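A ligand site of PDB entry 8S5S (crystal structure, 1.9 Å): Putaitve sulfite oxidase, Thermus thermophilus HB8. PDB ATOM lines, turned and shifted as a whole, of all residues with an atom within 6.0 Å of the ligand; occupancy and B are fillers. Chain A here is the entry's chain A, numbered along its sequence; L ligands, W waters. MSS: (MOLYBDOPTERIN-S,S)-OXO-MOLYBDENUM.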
ATOM      1  N   LEU A  47     -26.266  -6.776  -3.644  1.00  0.00           N
ATOM      2  CA  LEU A  47     -26.424  -6.505  -2.219  1.00  0.00           C
ATOM      3  C   LEU A  47     -25.072  -6.270  -1.549  1.00  0.00           C
ATOM      4  O   LEU A  47     -24.086  -6.988  -1.788  1.00  0.00           O
ATOM      5  CB  LEU A  47     -27.179  -7.655  -1.570  1.00  0.00           C
ATOM      6  CG  LEU A  47     -27.519  -7.529  -0.077  1.00  0.00           C
ATOM      7  CD1 LEU A  47     -28.454  -6.361   0.238  1.00  0.00           C
ATOM      8  CD2 LEU A  47     -28.163  -8.835   0.373  1.00  0.00           C
ATOM      9  N   TYR A  48     -24.987  -5.208  -0.713  1.00  0.00           N
ATOM     10  CA  TYR A  48     -23.777  -4.862   0.015  1.00  0.00           C
ATOM     11  C   TYR A  48     -23.333  -6.011   0.904  1.00  0.00           C
ATOM     12  O   TYR A  48     -24.077  -6.905   1.299  1.00  0.00           O
ATOM     13  CB  TYR A  48     -23.960  -3.563   0.818  1.00  0.00           C
ATOM     14  CG  TYR A  48     -24.627  -3.807   2.175  1.00  0.00           C
ATOM     15  CD1 TYR A  48     -26.018  -3.864   2.287  1.00  0.00           C
ATOM     16  CD2 TYR A  48     -23.890  -3.927   3.335  1.00  0.00           C
ATOM     17  CE1 TYR A  48     -26.635  -4.090   3.510  1.00  0.00           C
ATOM     18  CE2 TYR A  48     -24.498  -4.195   4.561  1.00  0.00           C
ATOM     19  CZ  TYR A  48     -25.881  -4.213   4.660  1.00  0.00           C
ATOM     20  OH  TYR A  48     -26.495  -4.444   5.871  1.00  0.00           O
ATOM     21  N   ILE A  49     -22.031  -6.014   1.197  1.00  0.00           N
ATOM     22  CA  ILE A  49     -21.439  -6.956   2.125  1.00  0.00           C
ATOM     23  C   ILE A  49     -20.662  -6.166   3.156  1.00  0.00           C
ATOM     24  O   ILE A  49     -19.914  -5.263   2.805  1.00  0.00           O
ATOM     25  CB  ILE A  49     -20.466  -7.916   1.435  1.00  0.00           C
ATOM     26  CG1 ILE A  49     -21.090  -8.648   0.298  1.00  0.00           C
ATOM     27  CG2 ILE A  49     -19.850  -8.876   2.462  1.00  0.00           C
ATOM     28  CD1 ILE A  49     -22.056  -9.724   0.742  1.00  0.00           C
ATOM     29  N   ARG A  50     -20.817  -6.552   4.413  1.00  0.00           N
ATOM     30  CA  ARG A  50     -19.950  -6.092   5.487  1.00  0.00           C
ATOM     31  C   ARG A  50     -19.683  -7.276   6.418  1.00  0.00           C
ATOM     32  O   ARG A  50     -20.535  -7.644   7.254  1.00  0.00           O
ATOM     33  CB  ARG A  50     -20.587  -4.904   6.214  1.00  0.00           C
ATOM     34  CG  ARG A  50     -19.607  -4.129   7.081  1.00  0.00           C
ATOM     35  CD  ARG A  50     -19.201  -4.867   8.348  1.00  0.00           C
ATOM     36  NE  ARG A  50     -18.716  -3.936   9.361  1.00  0.00           N
ATOM     37  CZ  ARG A  50     -17.425  -3.740   9.685  1.00  0.00           C
ATOM     38  NH1 ARG A  50     -16.474  -4.481   9.178  1.00  0.00           N
ATOM     39  NH2 ARG A  50     -17.084  -2.795  10.535  1.00  0.00           N
ATOM     40  N   ASN A  51     -18.505  -7.848   6.262  1.00  0.00           N
ATOM     41  CA  ASN A  51     -17.969  -8.748   7.283  1.00  0.00           C
ATOM     42  C   ASN A  51     -17.046  -7.980   8.231  1.00  0.00           C
ATOM     43  O   ASN A  51     -16.155  -7.279   7.739  1.00  0.00           O
ATOM     44  CB  ASN A  51     -17.204  -9.874   6.623  1.00  0.00           C
ATOM     45  CG  ASN A  51     -18.119 -10.819   5.872  1.00  0.00           C
ATOM     46  OD1 ASN A  51     -19.319 -10.931   6.191  1.00  0.00           O
ATOM     47  ND2 ASN A  51     -17.540 -11.520   4.917  1.00  0.00           N
ATOM     48  N   ASN A  52     -17.355  -8.034   9.552  1.00  0.00           N
ATOM     49  CA  ASN A  52     -16.373  -7.777  10.596  1.00  0.00           C
ATOM     50  C   ASN A  52     -15.412  -8.952  10.635  1.00  0.00           C
ATOM     51  O   ASN A  52     -14.186  -8.799  10.683  1.00  0.00           O
ATOM     52  CB  ASN A  52     -16.935  -7.656  12.013  1.00  0.00           C
ATOM     53  CG  ASN A  52     -17.881  -6.488  12.231  1.00  0.00           C
ATOM     54  OD1 ASN A  52     -17.518  -5.497  12.897  1.00  0.00           O
ATOM     55  ND2 ASN A  52     -19.095  -6.599  11.692  1.00  0.00           N
ATOM     56  N   VAL A  53     -15.985 -10.161  10.644  1.00  0.00           N
ATOM     57  CA  VAL A  53     -15.205 -11.396  10.743  1.00  0.00           C
ATOM     58  C   VAL A  53     -15.550 -12.283   9.548  1.00  0.00           C
ATOM     59  O   VAL A  53     -16.667 -12.800   9.483  1.00  0.00           O
ATOM     60  CB  VAL A  53     -15.446 -12.183  12.052  1.00  0.00           C
ATOM     61  CG1 VAL A  53     -14.636 -13.481  12.074  1.00  0.00           C
ATOM     62  CG2 VAL A  53     -15.187 -11.365  13.328  1.00  0.00           C
ATOM     63  N   ASP A  54     -14.568 -12.505   8.647  1.00  0.00           N
ATOM     64  CA  ASP A  54     -14.730 -13.437   7.528  1.00  0.00           C
ATOM     65  C   ASP A  54     -14.880 -14.882   8.020  1.00  0.00           C
ATOM     66  O   ASP A  54     -14.151 -15.302   8.902  1.00  0.00           O
ATOM     67  CB  ASP A  54     -13.547 -13.336   6.581  1.00  0.00           C
ATOM     68  CG  ASP A  54     -13.441 -12.006   5.840  1.00  0.00           C
ATOM     69  OD1 ASP A  54     -14.487 -11.309   5.749  1.00  0.00           O
ATOM     70  OD2 ASP A  54     -12.335 -11.683   5.334  1.00  0.00           O
ATOM     71  N   LEU A 100     -32.294  -4.288   5.267  1.00  0.00           N
ATOM     72  CA  LEU A 100     -31.051  -4.731   5.839  1.00  0.00           C
ATOM     73  C   LEU A 100     -30.078  -3.604   5.613  1.00  0.00           C
ATOM     74  O   LEU A 100     -29.768  -3.287   4.489  1.00  0.00           O
ATOM     75  CB  LEU A 100     -30.601  -6.028   5.189  1.00  0.00           C
ATOM     76  CG  LEU A 100     -29.299  -6.639   5.709  1.00  0.00           C
ATOM     77  CD1 LEU A 100     -29.420  -7.084   7.147  1.00  0.00           C
ATOM     78  CD2 LEU A 100     -28.898  -7.800   4.781  1.00  0.00           C
ATOM     79  N   GLN A 101     -29.697  -2.919   6.684  1.00  0.00           N
ATOM     80  CA  GLN A 101     -28.944  -1.686   6.583  1.00  0.00           C
ATOM     81  C   GLN A 101     -27.803  -1.758   7.571  1.00  0.00           C
ATOM     82  O   GLN A 101     -27.989  -2.075   8.745  1.00  0.00           O
ATOM     83  CB  GLN A 101     -29.677  -0.396   6.923  1.00  0.00           C
ATOM     84  CG  GLN A 101     -28.879   0.830   6.508  1.00  0.00           C
ATOM     85  CD  GLN A 101     -29.589   2.130   6.709  1.00  0.00           C
ATOM     86  OE1 GLN A 101     -29.268   3.137   6.081  1.00  0.00           O
ATOM     87  NE2 GLN A 101     -30.590   2.143   7.592  1.00  0.00           N
ATOM     88  N   CYS A 102     -26.609  -1.388   7.087  1.00  0.00           N
ATOM     89  CA  CYS A 102     -25.451  -1.327   7.966  1.00  0.00           C
ATOM     90  C   CYS A 102     -25.635  -0.148   8.901  1.00  0.00           C
ATOM     91  O   CYS A 102     -26.008   0.929   8.452  1.00  0.00           O
ATOM     92  CB  CYS A 102     -24.134  -1.181   7.196  1.00  0.00           C
ATOM     93  SG  CYS A 102     -22.665  -1.342   8.255  1.00  0.00           S
ATOM     94  N   SER A 103     -25.234  -0.311  10.172  1.00  0.00           N
ATOM     95  CA  SER A 103     -25.305   0.800  11.109  1.00  0.00           C
ATOM     96  C   SER A 103     -24.312   1.866  10.654  1.00  0.00           C
ATOM     97  O   SER A 103     -24.391   3.016  11.049  1.00  0.00           O
ATOM     98  CB  SER A 103     -25.039   0.345  12.549  1.00  0.00           C
ATOM     99  OG  SER A 103     -23.718  -0.177  12.680  1.00  0.00           O
ATOM    100  N   GLY A 104     -23.354   1.502   9.793  1.00  0.00           N
ATOM    101  CA  GLY A 104     -22.418   2.491   9.312  1.00  0.00           C
ATOM    102  C   GLY A 104     -22.861   3.133   8.016  1.00  0.00           C
ATOM    103  O   GLY A 104     -22.186   4.046   7.563  1.00  0.00           O
ATOM    104  N   ALA A 156     -21.756 -16.218  16.236  1.00  0.00           N
ATOM    105  CA  ALA A 156     -21.429 -16.789  14.942  1.00  0.00           C
ATOM    106  C   ALA A 156     -20.503 -17.986  15.122  1.00  0.00           C
ATOM    107  O   ALA A 156     -19.770 -18.109  16.101  1.00  0.00           O
ATOM    108  CB  ALA A 156     -20.771 -15.722  14.087  1.00  0.00           C
ATOM    109  N   SER A 157     -20.528 -18.862  14.105  1.00  0.00           N
ATOM    110  CA  SER A 157     -19.579 -19.944  13.957  1.00  0.00           C
ATOM    111  C   SER A 157     -18.135 -19.461  14.142  1.00  0.00           C
ATOM    112  O   SER A 157     -17.739 -18.405  13.649  1.00  0.00           O
ATOM    113  CB  SER A 157     -19.757 -20.577  12.593  1.00  0.00           C
ATOM    114  OG  SER A 157     -18.883 -21.679  12.479  1.00  0.00           O
ATOM    115  N   PHE A 165     -17.951 -13.525  17.048  1.00  0.00           N
ATOM    116  CA  PHE A 165     -18.810 -12.402  16.720  1.00  0.00           C
ATOM    117  C   PHE A 165     -20.111 -12.630  17.472  1.00  0.00           C
ATOM    118  O   PHE A 165     -20.815 -13.602  17.188  1.00  0.00           O
ATOM    119  CB  PHE A 165     -19.077 -12.275  15.211  1.00  0.00           C
ATOM    120  CG  PHE A 165     -19.797 -10.970  14.891  1.00  0.00           C
ATOM    121  CD1 PHE A 165     -19.107  -9.777  14.826  1.00  0.00           C
ATOM    122  CD2 PHE A 165     -21.207 -10.957  14.767  1.00  0.00           C
ATOM    123  CE1 PHE A 165     -19.788  -8.601  14.550  1.00  0.00           C
ATOM    124  CE2 PHE A 165     -21.876  -9.763  14.527  1.00  0.00           C
ATOM    125  CZ  PHE A 165     -21.170  -8.603  14.456  1.00  0.00           C
ATOM    126  N   VAL A 191     -22.067 -15.912   1.591  1.00  0.00           N
ATOM    127  CA  VAL A 191     -21.436 -14.673   1.986  1.00  0.00           C
ATOM    128  C   VAL A 191     -22.426 -13.804   2.777  1.00  0.00           C
ATOM    129  O   VAL A 191     -21.989 -12.882   3.459  1.00  0.00           O
ATOM    130  CB  VAL A 191     -20.885 -13.879   0.799  1.00  0.00           C
ATOM    131  CG1 VAL A 191     -22.002 -13.224  -0.023  1.00  0.00           C
ATOM    132  CG2 VAL A 191     -19.873 -12.859   1.275  1.00  0.00           C
ATOM    133  N   HIS A 192     -23.729 -14.104   2.701  1.00  0.00           N
ATOM    134  CA  HIS A 192     -24.733 -13.375   3.432  1.00  0.00           C
ATOM    135  C   HIS A 192     -25.188 -14.185   4.644  1.00  0.00           C
ATOM    136  O   HIS A 192     -26.241 -13.907   5.168  1.00  0.00           O
ATOM    137  CB  HIS A 192     -25.919 -13.003   2.520  1.00  0.00           C
ATOM    138  CG  HIS A 192     -25.539 -11.941   1.535  1.00  0.00           C
ATOM    139  ND1 HIS A 192     -25.246 -10.625   1.860  1.00  0.00           N
ATOM    140  CD2 HIS A 192     -25.392 -12.031   0.201  1.00  0.00           C
ATOM    141  CE1 HIS A 192     -24.927  -9.977   0.760  1.00  0.00           C
ATOM    142  NE2 HIS A 192     -25.033 -10.792  -0.263  1.00  0.00           N
ATOM    143  N   GLY A 193     -24.443 -15.236   5.006  1.00  0.00           N
ATOM    144  CA  GLY A 193     -24.640 -15.969   6.244  1.00  0.00           C
ATOM    145  C   GLY A 193     -25.172 -17.376   6.059  1.00  0.00           C
ATOM    146  O   GLY A 193     -25.480 -18.048   7.048  1.00  0.00           O
ATOM    147  N   ARG A 197     -28.816 -17.825   9.211  1.00  0.00           N
ATOM    148  CA  ARG A 197     -28.567 -16.525   9.797  1.00  0.00           C
ATOM    149  C   ARG A 197     -29.715 -16.190  10.718  1.00  0.00           C
ATOM    150  O   ARG A 197     -30.864 -16.474  10.390  1.00  0.00           O
ATOM    151  CB  ARG A 197     -28.365 -15.499   8.698  1.00  0.00           C
ATOM    152  CG  ARG A 197     -28.242 -14.029   9.089  1.00  0.00           C
ATOM    153  CD  ARG A 197     -28.051 -13.124   7.893  1.00  0.00           C
ATOM    154  NE  ARG A 197     -27.412 -11.890   8.299  1.00  0.00           N
ATOM    155  CZ  ARG A 197     -26.901 -10.981   7.496  1.00  0.00           C
ATOM    156  NH1 ARG A 197     -26.937 -11.172   6.205  1.00  0.00           N
ATOM    157  NH2 ARG A 197     -26.377  -9.884   7.986  1.00  0.00           N
ATOM    158  N   PHE A 204     -30.592  -3.023  12.881  1.00  0.00           N
ATOM    159  CA  PHE A 204     -29.422  -2.839  12.055  1.00  0.00           C
ATOM    160  C   PHE A 204     -28.715  -4.157  11.813  1.00  0.00           C
ATOM    161  O   PHE A 204     -28.742  -5.116  12.590  1.00  0.00           O
ATOM    162  CB  PHE A 204     -28.440  -1.802  12.633  1.00  0.00           C
ATOM    163  CG  PHE A 204     -28.825  -0.362  12.441  1.00  0.00           C
ATOM    164  CD1 PHE A 204     -28.795   0.214  11.162  1.00  0.00           C
ATOM    165  CD2 PHE A 204     -29.241   0.430  13.515  1.00  0.00           C
ATOM    166  CE1 PHE A 204     -29.118   1.541  10.991  1.00  0.00           C
ATOM    167  CE2 PHE A 204     -29.538   1.772  13.345  1.00  0.00           C
ATOM    168  CZ  PHE A 204     -29.491   2.324  12.080  1.00  0.00           C
ATOM    169  N   GLY A 205     -28.092  -4.195  10.639  1.00  0.00           N
ATOM    170  CA  GLY A 205     -27.427  -5.357  10.090  1.00  0.00           C
ATOM    171  C   GLY A 205     -26.491  -6.102  11.053  1.00  0.00           C
ATOM    172  O   GLY A 205     -26.507  -7.326  11.036  1.00  0.00           O
ATOM    173  N   VAL A 206     -25.736  -5.358  11.861  1.00  0.00           N
ATOM    174  CA  VAL A 206     -24.749  -5.924  12.786  1.00  0.00           C
ATOM    175  C   VAL A 206     -25.394  -6.982  13.680  1.00  0.00           C
ATOM    176  O   VAL A 206     -24.742  -7.966  14.053  1.00  0.00           O
ATOM    177  CB  VAL A 206     -24.091  -4.803  13.609  1.00  0.00           C
ATOM    178  CG1 VAL A 206     -25.092  -4.117  14.546  1.00  0.00           C
ATOM    179  CG2 VAL A 206     -22.908  -5.329  14.424  1.00  0.00           C
ATOM    180  N   ASN A 207     -26.662  -6.769  14.011  1.00  0.00           N
ATOM    181  CA  ASN A 207     -27.364  -7.679  14.887  1.00  0.00           C
ATOM    182  C   ASN A 207     -27.803  -8.973  14.239  1.00  0.00           C
ATOM    183  O   ASN A 207     -28.163  -9.909  14.946  1.00  0.00           O
ATOM    184  CB  ASN A 207     -28.601  -7.008  15.474  1.00  0.00           C
ATOM    185  CG  ASN A 207     -28.218  -5.749  16.191  1.00  0.00           C
ATOM    186  OD1 ASN A 207     -27.498  -5.789  17.214  1.00  0.00           O
ATOM    187  ND2 ASN A 207     -28.582  -4.593  15.667  1.00  0.00           N
ATOM    188  N   ASN A 208     -27.863  -9.001  12.901  1.00  0.00           N
ATOM    189  CA  ASN A 208     -28.414 -10.148  12.180  1.00  0.00           C
ATOM    190  C   ASN A 208     -27.260 -11.118  11.928  1.00  0.00           C
ATOM    191  O   ASN A 208     -26.532 -10.952  10.955  1.00  0.00           O
ATOM    192  CB  ASN A 208     -29.024  -9.653  10.864  1.00  0.00           C
ATOM    193  CG  ASN A 208     -30.235  -8.768  11.093  1.00  0.00           C
ATOM    194  OD1 ASN A 208     -31.345  -9.271  11.135  1.00  0.00           O
ATOM    195  ND2 ASN A 208     -30.065  -7.483  11.318  1.00  0.00           N
ATOM    196  N   VAL A 209     -27.024 -12.029  12.862  1.00  0.00           N
ATOM    197  CA  VAL A 209     -25.780 -12.761  12.974  1.00  0.00           C
ATOM    198  C   VAL A 209     -25.707 -13.887  11.926  1.00  0.00           C
ATOM    199  O   VAL A 209     -26.484 -14.818  11.943  1.00  0.00           O
ATOM    200  CB  VAL A 209     -25.599 -13.331  14.388  1.00  0.00           C
ATOM    201  CG1 VAL A 209     -24.376 -14.258  14.437  1.00  0.00           C
ATOM    202  CG2 VAL A 209     -25.513 -12.200  15.409  1.00  0.00           C
ATOM    203  N   LYS A 210     -24.754 -13.739  10.999  1.00  0.00           N
ATOM    204  CA  LYS A 210     -24.524 -14.739   9.976  1.00  0.00           C
ATOM    205  C   LYS A 210     -23.873 -15.995  10.564  1.00  0.00           C
ATOM    206  O   LYS A 210     -23.162 -15.918  11.554  1.00  0.00           O
ATOM    207  CB  LYS A 210     -23.536 -14.169   8.967  1.00  0.00           C
ATOM    208  CG  LYS A 210     -23.958 -12.930   8.199  1.00  0.00           C
ATOM    209  CD  LYS A 210     -22.785 -12.359   7.397  1.00  0.00           C
ATOM    210  CE  LYS A 210     -23.051 -11.197   6.569  1.00  0.00           C
ATOM    211  NZ  LYS A 210     -21.906 -10.886   5.664  1.00  0.00           N
ATOM    212  N   TRP A 211     -24.137 -17.155   9.951  1.00  0.00           N
ATOM    213  CA  TRP A 211     -23.508 -18.402  10.364  1.00  0.00           C
ATOM    214  C   TRP A 211     -23.765 -18.687  11.844  1.00  0.00           C
ATOM    215  O   TRP A 211     -22.839 -19.061  12.599  1.00  0.00           O
ATOM    216  CB  TRP A 211     -22.015 -18.377  10.059  1.00  0.00           C
ATOM    217  CG  TRP A 211     -21.712 -17.875   8.680  1.00  0.00           C
ATOM    218  CD1 TRP A 211     -22.168 -18.401   7.519  1.00  0.00           C
ATOM    219  CD2 TRP A 211     -20.979 -16.683   8.339  1.00  0.00           C
ATOM    220  NE1 TRP A 211     -21.781 -17.619   6.472  1.00  0.00           N
ATOM    221  CE2 TRP A 211     -21.010 -16.589   6.916  1.00  0.00           C
ATOM    222  CE3 TRP A 211     -20.251 -15.731   9.052  1.00  0.00           C
ATOM    223  CZ2 TRP A 211     -20.391 -15.562   6.214  1.00  0.00           C
ATOM    224  CZ3 TRP A 211     -19.641 -14.704   8.355  1.00  0.00           C
ATOM    225  CH2 TRP A 211     -19.707 -14.637   6.957  1.00  0.00           C
ATOM    226  N   TYR A 231     -20.320  -0.317  18.114  1.00  0.00           N
ATOM    227  CA  TYR A 231     -21.719  -0.429  17.697  1.00  0.00           C
ATOM    228  C   TYR A 231     -22.609   0.173  18.751  1.00  0.00           C
ATOM    229  O   TYR A 231     -23.661  -0.394  19.131  1.00  0.00           O
ATOM    230  CB  TYR A 231     -22.068  -1.889  17.395  1.00  0.00           C
ATOM    231  CG  TYR A 231     -21.279  -2.363  16.192  1.00  0.00           C
ATOM    232  CD1 TYR A 231     -21.594  -1.897  14.923  1.00  0.00           C
ATOM    233  CD2 TYR A 231     -20.252  -3.296  16.306  1.00  0.00           C
ATOM    234  CE1 TYR A 231     -20.863  -2.289  13.805  1.00  0.00           C
ATOM    235  CE2 TYR A 231     -19.577  -3.755  15.183  1.00  0.00           C
ATOM    236  CZ  TYR A 231     -19.861  -3.220  13.935  1.00  0.00           C
ATOM    237  OH  TYR A 231     -19.172  -3.582  12.802  1.00  0.00           O
ATOM    238  N   ASN A 262     -26.454  -0.036  18.567  1.00  0.00           N
ATOM    239  CA  ASN A 262     -27.109   0.063  17.273  1.00  0.00           C
ATOM    240  C   ASN A 262     -28.122  -1.074  17.163  1.00  0.00           C
ATOM    241  O   ASN A 262     -27.768  -2.202  16.891  1.00  0.00           O
ATOM    242  CB  ASN A 262     -26.140  -0.008  16.114  1.00  0.00           C
ATOM    243  CG  ASN A 262     -25.007   0.965  16.156  1.00  0.00           C
ATOM    244  OD1 ASN A 262     -23.952   0.593  15.670  1.00  0.00           O
ATOM    245  ND2 ASN A 262     -25.191   2.163  16.700  1.00  0.00           N
HETATM  246  N1  MSS L   1     -22.600 -11.789  11.285  1.00  0.00           N
HETATM  247  C2  MSS L   1     -21.328 -12.370  11.480  1.00  0.00           C
HETATM  248  N2  MSS L   1     -21.278 -13.667  11.853  1.00  0.00           N
HETATM  249  N3  MSS L   1     -20.122 -11.772  11.311  1.00  0.00           N
HETATM  250  C4  MSS L   1     -20.051 -10.454  10.940  1.00  0.00           C
HETATM  251  O4  MSS L   1     -18.953  -9.816  10.781  1.00  0.00           O
HETATM  252  N5  MSS L   1     -21.310  -8.452  10.303  1.00  0.00           N
HETATM  253  C6  MSS L   1     -22.560  -7.730  10.529  1.00  0.00           C
HETATM  254  C7  MSS L   1     -23.844  -8.555  10.176  1.00  0.00           C
HETATM  255  N8  MSS L   1     -23.820  -9.898  10.709  1.00  0.00           N
HETATM  256  C9  MSS L   1     -21.326  -9.775  10.668  1.00  0.00           C
HETATM  257  C10 MSS L   1     -22.627 -10.508  10.893  1.00  0.00           C
HETATM  258  C1' MSS L   1     -22.689  -6.339   9.972  1.00  0.00           C
HETATM  259  S1' MSS L   1     -21.828  -5.074  10.742  1.00  0.00           S
HETATM  260  C2' MSS L   1     -23.562  -6.070   8.952  1.00  0.00           C
HETATM  261  S2' MSS L   1     -23.900  -4.490   8.428  1.00  0.00           S
HETATM  262  C3' MSS L   1     -24.314  -7.195   8.283  1.00  0.00           C
HETATM  263  O3' MSS L   1     -24.007  -8.495   8.753  1.00  0.00           O
HETATM  264  C4' MSS L   1     -23.979  -7.283   6.852  1.00  0.00           C
HETATM  265  O4' MSS L   1     -24.950  -8.094   6.182  1.00  0.00           O
HETATM  266  P   MSS L   1     -24.500  -8.485   4.618  1.00  0.00           P
HETATM  267  O1P MSS L   1     -25.289  -9.718   4.427  1.00  0.00           O
HETATM  268  O2P MSS L   1     -22.831  -8.623   4.784  1.00  0.00           O
HETATM  269  O3P MSS L   1     -25.219  -7.357   3.763  1.00  0.00           O
HETATM  270 MOM1 MSS L   1     -22.808  -3.043  10.038  1.00  0.00          MO
HETATM  271  OM1 MSS L   1     -24.316  -2.747  11.164  1.00  0.00           O
HETATM  272  O   HOH W   1     -20.934  -2.205  10.261  1.00  0.00           O
HETATM  273  O   HOH W   2     -18.329 -14.124  11.896  1.00  0.00           O
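Water W1 lies within hydrogen-bond range of NE of Arg 50 (3.0 Å) and OH of Tyr 231 (3.4 Å). Water W2 bridges a nitrogen (N2) of the ligand (3.0 Å) and the backbone carbonyl oxygen of Val 53 (3.2 Å).
N of Ser 103 lies close to OM1 of the ligand. N of Val 206 lies close to OM1 of the ligand, 3.1 Å away. Residues that only touch the ligand: Gly 205, Ala 156, Ile 49, Phe 165, Trp 211, Asn 51, Val 209 and Leu 100. Hydrophobic or aromatic side chains within 4 Å of the ligand: Tyr 48, Ile 49, Leu 100, Ala 156, Phe 165, His 192, Val 206 and Trp 211. Within 4 Å of the ligand: Tyr 48, Ile 49, Arg 50, Asn 51, Asn 52, Val 53, Leu 100, Cys 102, Ser 103, Ala 156, Phe 165, His 192, Arg 197, Gly 205, Val 206, Asn 208, Val 209, Lys 210, Trp 211 and Tyr 231. The nearest printed residue that does not touch the ligand is Gln 101 (4.4 Å).
N of Cys 102 sits at hydrogen-bond distance from OH of Tyr 48 (3.3 Å). O of Val 191 is in hydrogen-bond range of NZ of Lys 210 (3.0 Å). OD1 of Asn 52 sits at hydrogen-bond distance from OH of Tyr 231 (2.5 Å). O of His 192 sits at hydrogen-bond distance from NH1 of Arg 197 (3.0 Å). OG of Ser 103 is in hydrogen-bond range of OD1 of Asn 262, at 3.1 Å. The guanidinium group of Arg 197 is in hydrogen-bond range of the backbone carbonyl oxygen of Asn 208 (3.0 Å). The guanidinium group (NH2) of Arg 50 lies within hydrogen-bond range of the side-chain hydroxyl (OH) of Tyr 231, at 3.2 Å. O of Phe 204 sits at hydrogen-bond distance from ND2 of Asn 208, at 3.0 Å.
The side-chain sulfur of Cys 102 is bound to a molybdenum atom (MOM1) of the ligand (2.5 Å). The backbone NH (N) of Lys 210 is in hydrogen-bond range of a nitrogen (N1) of the ligand, 2.9 Å away. N2 of the ligand is in hydrogen-bond range of O of Lys 210, 3.0 Å away. The side-chain amino group (NZ) of Lys 210 is in salt-bridge range of an oxygen (O2P) of the ligand, 2.6 Å away. The backbone NH (N) of Asn 52 is in hydrogen-bond range of an oxygen (O4) of the ligand (2.7 Å). A nitrogen (N5) of the ligand lies close to the side-chain amide nitrogen of Asn 52 (3.2 Å). An oxygen (O1P) of the ligand is in hydrogen-bond range of a ring nitrogen (ND1) of His 192, 2.7 Å away. The backbone carbonyl oxygen (O) of Tyr 48 lies close to an oxygen (O3P) of the ligand, 2.8 Å away. OH of Tyr 48 sits close to S2' of the ligand (3.6 Å). An oxygen (O1P) of the ligand lies within salt-bridge range of the guanidinium group (NH1) of Arg 197, at 2.8 Å. O2P of the ligand lies within hydrogen-bond range of N of Arg 50. O of Arg 50 lies within hydrogen-bond range of N5 of the ligand (3.2 Å). A sulfur (S1') of the ligand sits close to the guanidinium group (NE) of Arg 50, 3.6 Å away. The backbone carbonyl oxygen (O) of Asn 208 lies within hydrogen-bond range of a nitrogen (N8) of the ligand (2.9 Å). The backbone NH (N) of Val 53 lies within hydrogen-bond range of an oxygen (O4) of the ligand, 3.0 Å away. S1' of the ligand sits close to OH of Tyr 231 (3.7 Å).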
